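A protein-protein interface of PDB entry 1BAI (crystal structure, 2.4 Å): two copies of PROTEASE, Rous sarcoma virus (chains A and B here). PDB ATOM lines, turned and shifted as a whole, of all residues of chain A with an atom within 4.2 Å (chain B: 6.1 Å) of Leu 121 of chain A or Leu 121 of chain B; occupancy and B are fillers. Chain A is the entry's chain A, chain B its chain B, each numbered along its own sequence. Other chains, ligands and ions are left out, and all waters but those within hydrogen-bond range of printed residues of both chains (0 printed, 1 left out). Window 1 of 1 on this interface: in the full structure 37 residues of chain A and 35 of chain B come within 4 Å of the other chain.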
ATOM      1  N   LEU A   1      -8.610 -30.529 -18.785  1.00  0.00           N
ATOM      2  CA  LEU A   1      -8.659 -29.199 -18.121  1.00  0.00           C
ATOM      3  C   LEU A   1      -8.807 -29.400 -16.598  1.00  0.00           C
ATOM      4  O   LEU A   1      -9.140 -30.507 -16.119  1.00  0.00           O
ATOM      5  CB  LEU A   1      -9.836 -28.362 -18.691  1.00  0.00           C
ATOM      6  CG  LEU A   1      -9.789 -26.833 -18.822  1.00  0.00           C
ATOM      7  CD1 LEU A   1      -8.525 -26.428 -19.653  1.00  0.00           C
ATOM      8  CD2 LEU A   1     -11.068 -26.310 -19.475  1.00  0.00           C
ATOM      9  N   ALA A   2      -8.523 -28.326 -15.862  1.00  0.00           N
ATOM     10  CA  ALA A   2      -8.581 -28.291 -14.417  1.00  0.00           C
ATOM     11  C   ALA A   2      -8.450 -26.807 -14.209  1.00  0.00           C
ATOM     12  O   ALA A   2      -7.572 -26.196 -14.792  1.00  0.00           O
ATOM     13  CB  ALA A   2      -7.391 -29.040 -13.812  1.00  0.00           C
ATOM     14  N   MET A   3      -9.390 -26.217 -13.479  1.00  0.00           N
ATOM     15  CA  MET A   3      -9.394 -24.780 -13.230  1.00  0.00           C
ATOM     16  C   MET A   3     -10.182 -24.447 -11.982  1.00  0.00           C
ATOM     17  O   MET A   3     -11.426 -24.433 -12.023  1.00  0.00           O
ATOM     18  CB  MET A   3     -10.036 -24.071 -14.418  1.00  0.00           C
ATOM     19  CG  MET A   3      -9.995 -22.545 -14.370  1.00  0.00           C
ATOM     20  SD  MET A   3     -10.622 -21.850 -15.934  1.00  0.00           S
ATOM     21  CE  MET A   3      -9.776 -22.934 -17.182  1.00  0.00           C
ATOM     22  N   MET A   5     -12.084 -22.609  -9.056  1.00  0.00           N
ATOM     23  CA  MET A   5     -12.961 -21.452  -9.099  1.00  0.00           C
ATOM     24  C   MET A   5     -12.386 -20.368  -8.190  1.00  0.00           C
ATOM     25  O   MET A   5     -12.046 -20.623  -7.033  1.00  0.00           O
ATOM     26  CB  MET A   5     -14.386 -21.818  -8.677  1.00  0.00           C
ATOM     27  CG  MET A   5     -15.151 -22.615  -9.737  1.00  0.00           C
ATOM     28  SD  MET A   5     -15.266 -21.664 -11.289  1.00  0.00           S
ATOM     29  CE  MET A   5     -13.722 -22.231 -12.144  1.00  0.00           C
ATOM     30  N   LEU A 119     -16.582 -31.933 -18.978  1.00  0.00           N
ATOM     31  CA  LEU A 119     -16.469 -31.219 -17.727  1.00  0.00           C
ATOM     32  C   LEU A 119     -17.537 -31.429 -16.640  1.00  0.00           C
ATOM     33  O   LEU A 119     -18.756 -31.385 -16.891  1.00  0.00           O
ATOM     34  CB  LEU A 119     -16.178 -29.726 -18.000  1.00  0.00           C
ATOM     35  CG  LEU A 119     -14.693 -29.338 -18.213  1.00  0.00           C
ATOM     36  CD1 LEU A 119     -14.131 -30.099 -19.350  1.00  0.00           C
ATOM     37  CD2 LEU A 119     -14.488 -27.858 -18.475  1.00  0.00           C
ATOM     38  N   ARG A 120     -17.037 -31.779 -15.449  1.00  0.00           N
ATOM     39  CA  ARG A 120     -17.814 -31.980 -14.229  1.00  0.00           C
ATOM     40  C   ARG A 120     -17.238 -30.882 -13.355  1.00  0.00           C
ATOM     41  O   ARG A 120     -16.054 -30.692 -13.351  1.00  0.00           O
ATOM     42  CB  ARG A 120     -17.463 -33.322 -13.564  1.00  0.00           C
ATOM     43  CG  ARG A 120     -15.916 -33.565 -13.413  1.00  0.00           C
ATOM     44  CD  ARG A 120     -15.502 -34.445 -12.221  1.00  0.00           C
ATOM     45  NE  ARG A 120     -14.673 -35.572 -12.656  1.00  0.00           N
ATOM     46  CZ  ARG A 120     -13.354 -35.534 -12.869  1.00  0.00           C
ATOM     47  NH1 ARG A 120     -12.670 -34.422 -12.670  1.00  0.00           N
ATOM     48  NH2 ARG A 120     -12.732 -36.587 -13.379  1.00  0.00           N
ATOM     49  N   LEU A 121     -18.076 -30.146 -12.659  1.00  0.00           N
ATOM     50  CA  LEU A 121     -17.673 -29.060 -11.757  1.00  0.00           C
ATOM     51  C   LEU A 121     -17.615 -29.854 -10.472  1.00  0.00           C
ATOM     52  O   LEU A 121     -18.583 -30.565 -10.183  1.00  0.00           O
ATOM     53  CB  LEU A 121     -18.806 -28.017 -11.755  1.00  0.00           C
ATOM     54  CG  LEU A 121     -19.157 -26.857 -10.846  1.00  0.00           C
ATOM     55  CD1 LEU A 121     -18.335 -25.569 -10.964  1.00  0.00           C
ATOM     56  CD2 LEU A 121     -20.568 -26.568 -11.286  1.00  0.00           C
ATOM     57  N   THR A 122     -16.496 -29.787  -9.739  1.00  0.00           N
ATOM     58  CA  THR A 122     -16.317 -30.603  -8.534  1.00  0.00           C
ATOM     59  C   THR A 122     -15.449 -29.983  -7.455  1.00  0.00           C
ATOM     60  O   THR A 122     -14.566 -29.194  -7.743  1.00  0.00           O
ATOM     61  CB  THR A 122     -15.610 -31.941  -8.923  1.00  0.00           C
ATOM     62  OG1 THR A 122     -15.308 -32.728  -7.752  1.00  0.00           O
ATOM     63  CG2 THR A 122     -14.288 -31.654  -9.683  1.00  0.00           C
ATOM     64  N   LEU B   1     -19.844 -32.648  -3.594  1.00  0.00           N
ATOM     65  CA  LEU B   1     -20.161 -31.850  -4.809  1.00  0.00           C
ATOM     66  C   LEU B   1     -19.197 -32.195  -5.991  1.00  0.00           C
ATOM     67  O   LEU B   1     -17.998 -31.880  -5.982  1.00  0.00           O
ATOM     68  CB  LEU B   1     -20.115 -30.343  -4.493  1.00  0.00           C
ATOM     69  CG  LEU B   1     -21.003 -29.270  -5.162  1.00  0.00           C
ATOM     70  CD1 LEU B   1     -21.454 -29.622  -6.572  1.00  0.00           C
ATOM     71  CD2 LEU B   1     -22.180 -29.046  -4.287  1.00  0.00           C
ATOM     72  N   ALA B   2     -19.770 -32.848  -6.999  1.00  0.00           N
ATOM     73  CA  ALA B   2     -19.092 -33.251  -8.204  1.00  0.00           C
ATOM     74  C   ALA B   2     -20.234 -33.395  -9.209  1.00  0.00           C
ATOM     75  O   ALA B   2     -20.870 -34.442  -9.295  1.00  0.00           O
ATOM     76  CB  ALA B   2     -18.363 -34.599  -7.994  1.00  0.00           C
ATOM     77  N   MET B   3     -20.558 -32.293  -9.866  1.00  0.00           N
ATOM     78  CA  MET B   3     -21.619 -32.240 -10.866  1.00  0.00           C
ATOM     79  C   MET B   3     -21.064 -32.340 -12.290  1.00  0.00           C
ATOM     80  O   MET B   3     -20.274 -31.522 -12.731  1.00  0.00           O
ATOM     81  CB  MET B   3     -22.430 -30.930 -10.722  1.00  0.00           C
ATOM     82  CG  MET B   3     -23.155 -30.788  -9.364  1.00  0.00           C
ATOM     83  SD  MET B   3     -24.072 -29.218  -8.992  1.00  0.00           S
ATOM     84  CE  MET B   3     -25.735 -29.782  -9.422  1.00  0.00           C
ATOM     85  N   THR B   4     -21.460 -33.364 -13.005  1.00  0.00           N
ATOM     86  CA  THR B   4     -21.009 -33.466 -14.357  1.00  0.00           C
ATOM     87  C   THR B   4     -21.930 -32.591 -15.207  1.00  0.00           C
ATOM     88  O   THR B   4     -23.146 -32.666 -15.085  1.00  0.00           O
ATOM     89  CB  THR B   4     -20.918 -34.944 -14.791  1.00  0.00           C
ATOM     90  OG1 THR B   4     -19.536 -35.308 -14.850  1.00  0.00           O
ATOM     91  CG2 THR B   4     -21.586 -35.215 -16.127  1.00  0.00           C
ATOM     92  N   MET B   5     -21.325 -31.737 -16.037  1.00  0.00           N
ATOM     93  CA  MET B   5     -22.028 -30.775 -16.909  1.00  0.00           C
ATOM     94  C   MET B   5     -22.747 -31.310 -18.133  1.00  0.00           C
ATOM     95  O   MET B   5     -22.129 -31.829 -19.056  1.00  0.00           O
ATOM     96  CB  MET B   5     -21.053 -29.664 -17.332  1.00  0.00           C
ATOM     97  CG  MET B   5     -20.433 -28.914 -16.145  1.00  0.00           C
ATOM     98  SD  MET B   5     -21.625 -27.985 -15.109  1.00  0.00           S
ATOM     99  CE  MET B   5     -22.481 -29.202 -14.171  1.00  0.00           C
ATOM    100  N   PRO B  11     -27.091 -27.297 -13.451  1.00  0.00           N
ATOM    101  CA  PRO B  11     -26.339 -27.529 -12.225  1.00  0.00           C
ATOM    102  C   PRO B  11     -27.119 -26.850 -11.151  1.00  0.00           C
ATOM    103  O   PRO B  11     -26.828 -25.712 -10.828  1.00  0.00           O
ATOM    104  CB  PRO B  11     -25.089 -26.728 -12.446  1.00  0.00           C
ATOM    105  CG  PRO B  11     -24.901 -26.778 -13.870  1.00  0.00           C
ATOM    106  CD  PRO B  11     -26.262 -26.538 -14.399  1.00  0.00           C
ATOM    107  N   LEU B  36     -25.629 -23.486  -9.993  1.00  0.00           N
ATOM    108  CA  LEU B  36     -24.192 -23.294  -9.838  1.00  0.00           C
ATOM    109  C   LEU B  36     -23.787 -22.459 -11.059  1.00  0.00           C
ATOM    110  O   LEU B  36     -23.949 -22.920 -12.192  1.00  0.00           O
ATOM    111  CB  LEU B  36     -23.513 -24.656  -9.896  1.00  0.00           C
ATOM    112  CG  LEU B  36     -23.751 -25.498  -8.634  1.00  0.00           C
ATOM    113  CD1 LEU B  36     -22.536 -26.422  -8.543  1.00  0.00           C
ATOM    114  CD2 LEU B  36     -23.911 -24.627  -7.302  1.00  0.00           C
ATOM    115  N   ASP B  37     -23.137 -21.318 -10.875  1.00  0.00           N
ATOM    116  CA  ASP B  37     -22.871 -20.469 -12.017  1.00  0.00           C
ATOM    117  C   ASP B  37     -21.470 -19.903 -12.070  1.00  0.00           C
ATOM    118  O   ASP B  37     -21.174 -18.920 -11.415  1.00  0.00           O
ATOM    119  CB  ASP B  37     -23.914 -19.343 -11.955  1.00  0.00           C
ATOM    120  CG  ASP B  37     -24.156 -18.654 -13.283  1.00  0.00           C
ATOM    121  OD1 ASP B  37     -24.035 -19.245 -14.373  1.00  0.00           O
ATOM    122  OD2 ASP B  37     -24.532 -17.490 -13.244  1.00  0.00           O
ATOM    123  N   THR B  38     -20.621 -20.470 -12.909  1.00  0.00           N
ATOM    124  CA  THR B  38     -19.245 -20.000 -13.030  1.00  0.00           C
ATOM    125  C   THR B  38     -19.155 -18.713 -13.773  1.00  0.00           C
ATOM    126  O   THR B  38     -18.109 -18.069 -13.757  1.00  0.00           O
ATOM    127  CB  THR B  38     -18.330 -20.995 -13.834  1.00  0.00           C
ATOM    128  OG1 THR B  38     -19.117 -21.705 -14.804  1.00  0.00           O
ATOM    129  CG2 THR B  38     -17.693 -21.998 -12.938  1.00  0.00           C
ATOM    130  N   LEU B 114     -18.707 -19.983  -4.640  1.00  0.00           N
ATOM    131  CA  LEU B 114     -18.366 -21.133  -5.500  1.00  0.00           C
ATOM    132  C   LEU B 114     -16.924 -21.514  -5.228  1.00  0.00           C
ATOM    133  O   LEU B 114     -16.564 -22.644  -5.443  1.00  0.00           O
ATOM    134  CB  LEU B 114     -18.507 -20.834  -7.017  1.00  0.00           C
ATOM    135  CG  LEU B 114     -19.230 -21.880  -7.878  1.00  0.00           C
ATOM    136  CD1 LEU B 114     -20.683 -21.527  -7.844  1.00  0.00           C
ATOM    137  CD2 LEU B 114     -18.782 -21.987  -9.274  1.00  0.00           C
ATOM    138  N   LEU B 119     -15.138 -25.646  -5.295  1.00  0.00           N
ATOM    139  CA  LEU B 119     -15.403 -26.088  -6.668  1.00  0.00           C
ATOM    140  C   LEU B 119     -14.369 -25.628  -7.709  1.00  0.00           C
ATOM    141  O   LEU B 119     -13.724 -24.573  -7.556  1.00  0.00           O
ATOM    142  CB  LEU B 119     -16.842 -25.741  -7.089  1.00  0.00           C
ATOM    143  CG  LEU B 119     -17.897 -26.857  -6.961  1.00  0.00           C
ATOM    144  CD1 LEU B 119     -17.787 -27.502  -5.648  1.00  0.00           C
ATOM    145  CD2 LEU B 119     -19.308 -26.393  -7.259  1.00  0.00           C
ATOM    146  N   ARG B 120     -14.094 -26.504  -8.683  1.00  0.00           N
ATOM    147  CA  ARG B 120     -13.138 -26.193  -9.744  1.00  0.00           C
ATOM    148  C   ARG B 120     -13.605 -27.059 -10.914  1.00  0.00           C
ATOM    149  O   ARG B 120     -14.138 -28.140 -10.664  1.00  0.00           O
ATOM    150  CB  ARG B 120     -11.731 -26.607  -9.302  1.00  0.00           C
ATOM    151  CG  ARG B 120     -11.579 -28.094  -9.248  1.00  0.00           C
ATOM    152  CD  ARG B 120     -10.173 -28.639  -9.304  1.00  0.00           C
ATOM    153  NE  ARG B 120     -10.256 -30.098  -9.230  1.00  0.00           N
ATOM    154  CZ  ARG B 120     -10.693 -30.780  -8.159  1.00  0.00           C
ATOM    155  NH1 ARG B 120     -11.060 -30.143  -7.021  1.00  0.00           N
ATOM    156  NH2 ARG B 120     -10.903 -32.099  -8.262  1.00  0.00           N
ATOM    157  N   LEU B 121     -13.498 -26.584 -12.163  1.00  0.00           N
ATOM    158  CA  LEU B 121     -13.928 -27.402 -13.325  1.00  0.00           C
ATOM    159  C   LEU B 121     -12.817 -28.320 -13.810  1.00  0.00           C
ATOM    160  O   LEU B 121     -11.676 -27.895 -13.982  1.00  0.00           O
ATOM    161  CB  LEU B 121     -14.390 -26.563 -14.505  1.00  0.00           C
ATOM    162  CG  LEU B 121     -15.720 -25.822 -14.558  1.00  0.00           C
ATOM    163  CD1 LEU B 121     -16.393 -25.784 -13.250  1.00  0.00           C
ATOM    164  CD2 LEU B 121     -15.442 -24.455 -15.028  1.00  0.00           C
ATOM    165  N   THR B 122     -13.174 -29.538 -14.179  1.00  0.00           N
ATOM    166  CA  THR B 122     -12.160 -30.473 -14.587  1.00  0.00           C
ATOM    167  C   THR B 122     -12.680 -31.635 -15.435  1.00  0.00           C
ATOM    168  O   THR B 122     -13.870 -32.003 -15.398  1.00  0.00           O
ATOM    169  CB  THR B 122     -11.483 -31.018 -13.322  1.00  0.00           C
ATOM    170  OG1 THR B 122     -10.502 -32.008 -13.674  1.00  0.00           O
ATOM    171  CG2 THR B 122     -12.528 -31.604 -12.386  1.00  0.00           C
ATOM    172  N   ASN B 123     -11.768 -32.219 -16.193  1.00  0.00           N
ATOM    173  CA  ASN B 123     -12.109 -33.344 -17.033  1.00  0.00           C
ATOM    174  C   ASN B 123     -11.005 -34.362 -16.983  1.00  0.00           C
ATOM    175  O   ASN B 123     -10.849 -35.141 -17.905  1.00  0.00           O
ATOM    176  CB  ASN B 123     -12.374 -32.929 -18.486  1.00  0.00           C
ATOM    177  CG  ASN B 123     -11.212 -32.190 -19.115  1.00  0.00           C
ATOM    178  OD1 ASN B 123     -11.368 -31.066 -19.595  1.00  0.00           O
ATOM    179  ND2 ASN B 123     -10.043 -32.814 -19.141  1.00  0.00           N
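N of Leu 1 of chain A lies close to ND2 of Asn 123 of chain B, 2.7 Å away.
The backbone carbonyl oxygen (O) of Leu 119 of chain A lies within hydrogen-bond range of the backbone NH (N) of Met 5 of chain B, at 2.7 Å.
The backbone NH (N) of Leu 121 of chain A lies within hydrogen-bond range of the backbone carbonyl oxygen (O) of Met 3 of chain B.
O of Thr 122 of chain A sits at hydrogen-bond distance from N of Arg 120 of chain B.
The backbone NH of Arg 120 of chain A is in hydrogen-bond range of the backbone carbonyl oxygen of Thr 122 of chain B.
OG1 of Thr 122 of chain B lies within hydrogen-bond range of O of Leu 1 of chain A (3.2 Å).
O of Leu 1 of chain B sits close to OG1 of Thr 122 of chain A (3.3 Å).
The backbone NH of Met 5 of chain A is in hydrogen-bond range of the backbone carbonyl oxygen of Leu 119 of chain B (3.0 Å).
The backbone NH (N) of Met 3 of chain A is in hydrogen-bond range of the backbone carbonyl oxygen (O) of Leu 121 of chain B (2.9 Å).
The backbone carbonyl oxygen of Leu 114 of chain B lies within hydrogen-bond range of the backbone NH of Leu 119 of chain B, 3.3 Å away.
The backbone NH (N) of Leu 36 of chain B is in hydrogen-bond range of the backbone carbonyl oxygen (O) of Pro 11 of chain B, 2.7 Å away.
C of Thr 4 of chain B touches O of Leu 119 of chain A (3.8 Å).
Leu 119 of chain A touches Thr 122 of chain B (CA to O, 3.6 Å).
CD1 of Leu 119 of chain A touches OD1 of Asn 123 of chain B (2.9 Å).
CA of Arg 120 of chain A touches O of Met 3 of chain B (2.9 Å).
CA of Ala 2 of chain B touches O of Leu 121 of chain A, 3.4 Å away.
Leu 36 of chain B touches Leu 121 of chain A (CD1 to CD2, 3.4 Å).
Leu 114 of chain B touches Leu 121 of chain A (CD2 to CD1, 3.99 Å).
Leu 119 of chain B touches Leu 121 of chain A.
CD1 of Leu 121 of chain B touches CD1 of Leu 121 of chain A, 3.0 Å away.
Thr 122 of chain A touches Ala 2 of chain B (OG1 to CB, 3.6 Å).
Of the printed residues of chain B, Ala 2 of chain A touches Leu 121 (3.2 Å).
Printed residues of chain B within 4 Å of Leu 121 of chain A: Ala 2, Met 3, Leu 36, Leu 114, Leu 119, Arg 120 and Leu 121.
Of the printed residues of chain B, Thr 122 of chain A touches Leu 1 (3.3 Å), Ala 2 (3.6 Å), Leu 119 (3.4 Å), Arg 120 (2.9 Å) and Thr 122 (3.2 Å).
Of the printed residues of chain A, Ala 2 of chain B touches Leu 121 and Thr 122.
Pro 11 of chain B touches none of the printed residues of chain A.
Asp 37 of chain B touches none of the printed residues of chain A.
Printed residues of chain A within 4 Å of Leu 114 of chain B: Met 5 (3.7 Å) and Leu 121 (3.99 Å).
Of chain A, only Ala 2, Met 3, Arg 120 and Leu 121 come within 4 Å of Leu 121 of chain B.
The nearest printed residue of chain B that does not touch Leu 121 of chain A is Thr 38 of chain B (4.1 Å).
The nearest residue of chain A that does not touch Leu 121 of chain B is Met 5 of chain A (4.03 Å).
Hydrophobic or aromatic side chains of chain A within 4 Å of the printed part of chain B: Leu 1, Met 5, Leu 119 and Leu 121.
Hydrophobic or aromatic side chains of chain B that line the printed part of chain A: Ala 2, Met 3, Met 5, Leu 36, Leu 114, Leu 119 and Leu 121.
Among the printed residues, 30 pairs touch across the chains.
Among the printed residues, no Asp or Glu carboxylate lies within 4 Å of a Lys or Arg side-chain nitrogen of the other chain.
Ala 2 of chain A touches Leu 121 of chain B, and with the chains exchanged Leu 121 of chain A touches Ala 2 of chain B.
Met 3 of chain A touches Leu 121 of chain B, and with the chains exchanged Leu 121 of chain A touches Met 3 of chain B.
Leu 119 of chain A touches Thr 122 of chain B, and with the chains exchanged Thr 122 of chain A touches Leu 119 of chain B.
Thr 122 of chain A touches Ala 2 of chain B, but with the chains exchanged Ala 2 of chain A does not touch Thr 122 of chain B (4.1 Å).
8 positions are printed for both chains.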
